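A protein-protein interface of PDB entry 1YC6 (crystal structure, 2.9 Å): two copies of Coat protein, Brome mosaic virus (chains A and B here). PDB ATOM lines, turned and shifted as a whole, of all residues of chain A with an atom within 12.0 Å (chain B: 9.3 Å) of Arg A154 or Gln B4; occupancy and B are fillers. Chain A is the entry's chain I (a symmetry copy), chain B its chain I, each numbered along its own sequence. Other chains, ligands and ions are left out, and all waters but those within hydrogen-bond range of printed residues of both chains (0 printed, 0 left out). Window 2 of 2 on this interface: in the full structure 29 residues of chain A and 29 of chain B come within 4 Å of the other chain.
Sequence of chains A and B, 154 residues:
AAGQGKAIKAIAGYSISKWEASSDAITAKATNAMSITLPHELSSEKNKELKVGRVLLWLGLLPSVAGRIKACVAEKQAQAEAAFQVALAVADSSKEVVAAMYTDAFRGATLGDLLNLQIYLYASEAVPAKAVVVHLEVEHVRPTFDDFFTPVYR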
ATOM      1  N   PHE A 148     -13.217   0.427 -27.320  1.00  0.00           N
ATOM      2  CA  PHE A 148     -14.091  -0.444 -26.572  1.00  0.00           C
ATOM      3  C   PHE A 148     -14.640  -1.569 -27.402  1.00  0.00           C
ATOM      4  O   PHE A 148     -14.928  -1.401 -28.579  1.00  0.00           O
ATOM      5  CB  PHE A 148     -15.255   0.354 -25.983  1.00  0.00           C
ATOM      6  CG  PHE A 148     -14.826   1.464 -25.064  1.00  0.00           C
ATOM      7  CD1 PHE A 148     -14.552   2.735 -25.561  1.00  0.00           C
ATOM      8  CD2 PHE A 148     -14.661   1.231 -23.706  1.00  0.00           C
ATOM      9  CE1 PHE A 148     -14.120   3.754 -24.718  1.00  0.00           C
ATOM     10  CE2 PHE A 148     -14.228   2.250 -22.852  1.00  0.00           C
ATOM     11  CZ  PHE A 148     -13.959   3.510 -23.361  1.00  0.00           C
ATOM     12  N   PHE A 149     -14.773  -2.732 -26.784  1.00  0.00           N
ATOM     13  CA  PHE A 149     -15.348  -3.860 -27.480  1.00  0.00           C
ATOM     14  C   PHE A 149     -16.839  -3.566 -27.480  1.00  0.00           C
ATOM     15  O   PHE A 149     -17.290  -2.600 -26.853  1.00  0.00           O
ATOM     16  CB  PHE A 149     -15.128  -5.154 -26.696  1.00  0.00           C
ATOM     17  CG  PHE A 149     -13.778  -5.756 -26.873  1.00  0.00           C
ATOM     18  CD1 PHE A 149     -12.768  -5.523 -25.942  1.00  0.00           C
ATOM     19  CD2 PHE A 149     -13.511  -6.554 -27.981  1.00  0.00           C
ATOM     20  CE1 PHE A 149     -11.509  -6.074 -26.109  1.00  0.00           C
ATOM     21  CE2 PHE A 149     -12.264  -7.109 -28.164  1.00  0.00           C
ATOM     22  CZ  PHE A 149     -11.255  -6.870 -27.223  1.00  0.00           C
ATOM     23  N   THR A 150     -17.608  -4.382 -28.186  1.00  0.00           N
ATOM     24  CA  THR A 150     -19.045  -4.216 -28.153  1.00  0.00           C
ATOM     25  C   THR A 150     -19.412  -4.740 -26.742  1.00  0.00           C
ATOM     26  O   THR A 150     -18.764  -5.656 -26.222  1.00  0.00           O
ATOM     27  CB  THR A 150     -19.686  -5.037 -29.277  1.00  0.00           C
ATOM     28  OG1 THR A 150     -19.403  -4.401 -30.530  1.00  0.00           O
ATOM     29  CG2 THR A 150     -21.172  -5.147 -29.089  1.00  0.00           C
ATOM     30  N   PRO A 151     -20.416  -4.140 -26.082  1.00  0.00           N
ATOM     31  CA  PRO A 151     -20.769  -4.617 -24.737  1.00  0.00           C
ATOM     32  C   PRO A 151     -21.700  -5.823 -24.707  1.00  0.00           C
ATOM     33  O   PRO A 151     -22.887  -5.703 -24.427  1.00  0.00           O
ATOM     34  CB  PRO A 151     -21.395  -3.382 -24.097  1.00  0.00           C
ATOM     35  CG  PRO A 151     -22.091  -2.729 -25.270  1.00  0.00           C
ATOM     36  CD  PRO A 151     -21.100  -2.872 -26.402  1.00  0.00           C
ATOM     37  N   VAL A 152     -21.170  -7.001 -24.979  1.00  0.00           N
ATOM     38  CA  VAL A 152     -22.022  -8.166 -24.973  1.00  0.00           C
ATOM     39  C   VAL A 152     -22.227  -8.699 -23.570  1.00  0.00           C
ATOM     40  O   VAL A 152     -23.234  -9.340 -23.287  1.00  0.00           O
ATOM     41  CB  VAL A 152     -21.435  -9.254 -25.846  1.00  0.00           C
ATOM     42  CG1 VAL A 152     -21.358  -8.766 -27.284  1.00  0.00           C
ATOM     43  CG2 VAL A 152     -20.068  -9.634 -25.330  1.00  0.00           C
ATOM     44  N   TYR A 153     -21.284  -8.406 -22.683  1.00  0.00           N
ATOM     45  CA  TYR A 153     -21.339  -8.875 -21.292  1.00  0.00           C
ATOM     46  C   TYR A 153     -22.336  -8.194 -20.353  1.00  0.00           C
ATOM     47  O   TYR A 153     -21.954  -7.557 -19.368  1.00  0.00           O
ATOM     48  CB  TYR A 153     -19.934  -8.817 -20.696  1.00  0.00           C
ATOM     49  CG  TYR A 153     -19.057  -9.928 -21.215  1.00  0.00           C
ATOM     50  CD1 TYR A 153     -19.352 -10.555 -22.427  1.00  0.00           C
ATOM     51  CD2 TYR A 153     -17.960 -10.381 -20.484  1.00  0.00           C
ATOM     52  CE1 TYR A 153     -18.595 -11.605 -22.894  1.00  0.00           C
ATOM     53  CE2 TYR A 153     -17.181 -11.437 -20.943  1.00  0.00           C
ATOM     54  CZ  TYR A 153     -17.512 -12.047 -22.150  1.00  0.00           C
ATOM     55  OH  TYR A 153     -16.788 -13.128 -22.598  1.00  0.00           O
ATOM     56  N   ARG A 154     -23.620  -8.370 -20.648  1.00  0.00           N
ATOM     57  CA  ARG A 154     -24.685  -7.774 -19.844  1.00  0.00           C
ATOM     58  C   ARG A 154     -25.880  -8.715 -19.597  1.00  0.00           C
ATOM     59  O   ARG A 154     -26.065  -9.153 -18.431  1.00  0.00           O
ATOM     60  CB  ARG A 154     -25.167  -6.492 -20.529  1.00  0.00           C
ATOM     61  CG  ARG A 154     -24.136  -5.390 -20.550  1.00  0.00           C
ATOM     62  CD  ARG A 154     -23.735  -5.029 -19.132  1.00  0.00           C
ATOM     63  NE  ARG A 154     -22.713  -3.990 -19.116  1.00  0.00           N
ATOM     64  CZ  ARG A 154     -22.896  -2.756 -19.574  1.00  0.00           C
ATOM     65  NH1 ARG A 154     -24.068  -2.396 -20.085  1.00  0.00           N
ATOM     66  NH2 ARG A 154     -21.903  -1.880 -19.519  1.00  0.00           N
ATOM     67  OXT ARG A 154     -26.615  -9.001 -20.576  1.00  0.00           O
ATOM     68  N   ALA B   1     -16.161  -5.657 -12.256  1.00  0.00           N
ATOM     69  CA  ALA B   1     -17.161  -4.882 -13.051  1.00  0.00           C
ATOM     70  C   ALA B   1     -17.819  -3.766 -12.227  1.00  0.00           C
ATOM     71  O   ALA B   1     -18.993  -3.880 -11.858  1.00  0.00           O
ATOM     72  CB  ALA B   1     -18.237  -5.834 -13.601  1.00  0.00           C
ATOM     73  N   ALA B   2     -17.065  -2.695 -11.948  1.00  0.00           N
ATOM     74  CA  ALA B   2     -17.559  -1.539 -11.176  1.00  0.00           C
ATOM     75  C   ALA B   2     -18.489  -0.641 -12.021  1.00  0.00           C
ATOM     76  O   ALA B   2     -18.074   0.414 -12.525  1.00  0.00           O
ATOM     77  CB  ALA B   2     -16.369  -0.717 -10.639  1.00  0.00           C
ATOM     78  N   GLY B   3     -19.749  -1.067 -12.152  1.00  0.00           N
ATOM     79  CA  GLY B   3     -20.728  -0.339 -12.947  1.00  0.00           C
ATOM     80  C   GLY B   3     -20.980  -1.077 -14.255  1.00  0.00           C
ATOM     81  O   GLY B   3     -20.124  -1.083 -15.149  1.00  0.00           O
ATOM     82  N   GLN B   4     -22.147  -1.710 -14.373  1.00  0.00           N
ATOM     83  CA  GLN B   4     -22.481  -2.458 -15.587  1.00  0.00           C
ATOM     84  C   GLN B   4     -23.175  -1.594 -16.657  1.00  0.00           C
ATOM     85  O   GLN B   4     -24.184  -1.989 -17.256  1.00  0.00           O
ATOM     86  CB  GLN B   4     -23.339  -3.689 -15.235  1.00  0.00           C
ATOM     87  CG  GLN B   4     -22.900  -4.970 -15.968  1.00  0.00           C
ATOM     88  CD  GLN B   4     -21.420  -5.318 -15.739  1.00  0.00           C
ATOM     89  OE1 GLN B   4     -21.084  -6.149 -14.882  1.00  0.00           O
ATOM     90  NE2 GLN B   4     -20.532  -4.671 -16.503  1.00  0.00           N
ATOM     91  N   GLY B   5     -22.611  -0.407 -16.874  1.00  0.00           N
ATOM     92  CA  GLY B   5     -23.114   0.523 -17.865  1.00  0.00           C
ATOM     93  C   GLY B   5     -21.905   1.023 -18.635  1.00  0.00           C
ATOM     94  O   GLY B   5     -21.967   2.025 -19.341  1.00  0.00           O
ATOM     95  N   LYS B   6     -20.798   0.300 -18.484  1.00  0.00           N
ATOM     96  CA  LYS B   6     -19.530   0.623 -19.136  1.00  0.00           C
ATOM     97  C   LYS B   6     -19.058  -0.592 -19.919  1.00  0.00           C
ATOM     98  O   LYS B   6     -19.157  -1.726 -19.438  1.00  0.00           O
ATOM     99  CB  LYS B   6     -18.478   0.960 -18.088  1.00  0.00           C
ATOM    100  CG  LYS B   6     -18.982   1.885 -17.004  1.00  0.00           C
ATOM    101  CD  LYS B   6     -18.002   1.972 -15.852  1.00  0.00           C
ATOM    102  CE  LYS B   6     -18.512   2.911 -14.767  1.00  0.00           C
ATOM    103  NZ  LYS B   6     -17.490   3.130 -13.703  1.00  0.00           N
ATOM    104  N   ALA B   7     -18.538  -0.356 -21.119  1.00  0.00           N
ATOM    105  CA  ALA B   7     -18.051  -1.444 -21.958  1.00  0.00           C
ATOM    106  C   ALA B   7     -16.633  -1.821 -21.540  1.00  0.00           C
ATOM    107  O   ALA B   7     -16.003  -1.120 -20.737  1.00  0.00           O
ATOM    108  CB  ALA B   7     -18.078  -1.023 -23.422  1.00  0.00           C
ATOM    109  N   ILE B   8     -16.134  -2.934 -22.067  1.00  0.00           N
ATOM    110  CA  ILE B   8     -14.783  -3.371 -21.738  1.00  0.00           C
ATOM    111  C   ILE B   8     -13.792  -2.595 -22.626  1.00  0.00           C
ATOM    112  O   ILE B   8     -13.887  -2.610 -23.856  1.00  0.00           O
ATOM    113  CB  ILE B   8     -14.656  -4.926 -21.886  1.00  0.00           C
ATOM    114  CG1 ILE B   8     -13.235  -5.304 -22.304  1.00  0.00           C
ATOM    115  CG2 ILE B   8     -15.746  -5.458 -22.823  1.00  0.00           C
ATOM    116  CD1 ILE B   8     -12.178  -4.846 -21.329  1.00  0.00           C
ATOM    117  N   LYS B  95     -27.259 -19.674 -24.679  1.00  0.00           N
ATOM    118  CA  LYS B  95     -26.830 -19.042 -23.427  1.00  0.00           C
ATOM    119  C   LYS B  95     -27.362 -17.604 -23.311  1.00  0.00           C
ATOM    120  O   LYS B  95     -27.926 -17.055 -24.264  1.00  0.00           O
ATOM    121  CB  LYS B  95     -25.305 -19.013 -23.345  1.00  0.00           C
ATOM    122  CG  LYS B  95     -24.624 -20.345 -23.561  1.00  0.00           C
ATOM    123  CD  LYS B  95     -24.838 -21.283 -22.401  1.00  0.00           C
ATOM    124  CE  LYS B  95     -23.955 -22.519 -22.545  1.00  0.00           C
ATOM    125  NZ  LYS B  95     -24.281 -23.599 -21.556  1.00  0.00           N
ATOM    126  N   GLU B  96     -27.178 -17.005 -22.135  1.00  0.00           N
ATOM    127  CA  GLU B  96     -27.626 -15.635 -21.871  1.00  0.00           C
ATOM    128  C   GLU B  96     -26.824 -14.663 -22.696  1.00  0.00           C
ATOM    129  O   GLU B  96     -27.362 -13.723 -23.270  1.00  0.00           O
ATOM    130  CB  GLU B  96     -27.438 -15.287 -20.397  1.00  0.00           C
ATOM    131  CG  GLU B  96     -28.631 -15.636 -19.500  1.00  0.00           C
ATOM    132  CD  GLU B  96     -29.887 -14.792 -19.807  1.00  0.00           C
ATOM    133  OE1 GLU B  96     -29.797 -13.527 -19.772  1.00  0.00           O
ATOM    134  OE2 GLU B  96     -30.963 -15.405 -20.073  1.00  0.00           O
ATOM    135  N   VAL B  97     -25.517 -14.900 -22.726  1.00  0.00           N
ATOM    136  CA  VAL B  97     -24.583 -14.082 -23.487  1.00  0.00           C
ATOM    137  C   VAL B  97     -24.056 -14.926 -24.653  1.00  0.00           C
ATOM    138  O   VAL B  97     -23.305 -15.887 -24.443  1.00  0.00           O
ATOM    139  CB  VAL B  97     -23.405 -13.680 -22.608  1.00  0.00           C
ATOM    140  CG1 VAL B  97     -22.567 -12.623 -23.308  1.00  0.00           C
ATOM    141  CG2 VAL B  97     -23.917 -13.202 -21.256  1.00  0.00           C
ATOM    142  N   VAL B  98     -24.448 -14.578 -25.876  1.00  0.00           N
ATOM    143  CA  VAL B  98     -24.006 -15.337 -27.045  1.00  0.00           C
ATOM    144  C   VAL B  98     -22.724 -14.745 -27.598  1.00  0.00           C
ATOM    145  O   VAL B  98     -22.724 -14.109 -28.665  1.00  0.00           O
ATOM    146  CB  VAL B  98     -25.081 -15.328 -28.156  1.00  0.00           C
ATOM    147  CG1 VAL B  98     -24.619 -16.167 -29.365  1.00  0.00           C
ATOM    148  CG2 VAL B  98     -26.385 -15.863 -27.592  1.00  0.00           C
ATOM    149  N   ALA B  99     -21.630 -14.953 -26.875  1.00  0.00           N
ATOM    150  CA  ALA B  99     -20.347 -14.416 -27.300  1.00  0.00           C
ATOM    151  C   ALA B  99     -19.202 -15.254 -26.776  1.00  0.00           C
ATOM    152  O   ALA B  99     -19.358 -16.023 -25.829  1.00  0.00           O
ATOM    153  CB  ALA B  99     -20.190 -12.971 -26.822  1.00  0.00           C
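Hydrophobic or aromatic side chains of chain B within 4 Å of the printed part of chain A: Ala B7, Ile B8, Val B97 and Ala B99. Hydrophobic or aromatic side chains of chain A within 4 Å of the printed part of chain B: Phe A148, Phe A149, Val A152 and Tyr A153. Along chain A the printed residues that touch a printed residue of chain B span positions 148 to 154. Among the printed residues, 9 pairs touch across the chains. Among the printed residues, no Asp or Glu carboxylate lies within 4 Å of a Lys or Arg side-chain nitrogen of the other chain.
Of the printed residues of chain B, Phe A149 touches Ala B7 and Ile B8. Printed residues of chain B within 4 Å of Val A152: Val B97 (3.4 Å) and Ala B99 (3.7 Å). Of chain B, only Gln B4, Gly B5 and Lys B6 come within 4 Å of Arg A154. No residue of chain A comes within 4 Å of Ala B1. Of chain A, only Arg A154 (2.8 Å) comes within 4 Å of Gln B4. Gly B5 touches one residue of chain A. The nearest residue of chain B that does not touch Arg A154 is Ala B7 (4.03 Å). The nearest residue of chain A that does not touch Gln B4 is Tyr A153 (4.3 Å). The nearest printed residue of chain B that does not touch Val A152 is Val B98 (5.7 Å).
No position is printed for both chains.
O of Ile B8 is in hydrogen-bond range of N of Phe A149, 3.1 Å away. The backbone carbonyl oxygen (O) of Gln B4 lies close to the guanidinium group (NH1) of Arg A154, at 2.9 Å. The guanidinium group of Arg A154 sits close to the backbone NH of Gly B5. The backbone carbonyl oxygen (O) of Lys B6 sits at hydrogen-bond distance from the guanidinium group (NH2) of Arg A154.
Among the printed residues, pairs that only touch across the chains: Val A152 with Val B97 (3.4 Å), Phe A148 with Ile B8 (3.5 Å), Val A152 with Ala B99 (3.7 Å), Phe A149 with Ala B7 (3.9 Å) and Tyr A153 with Val B97 (3.9 Å).
The side-chain amino group (NZ) of Lys B6 sits at hydrogen-bond distance from the backbone carbonyl oxygen (O) of Ala B2 (3.0 Å).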
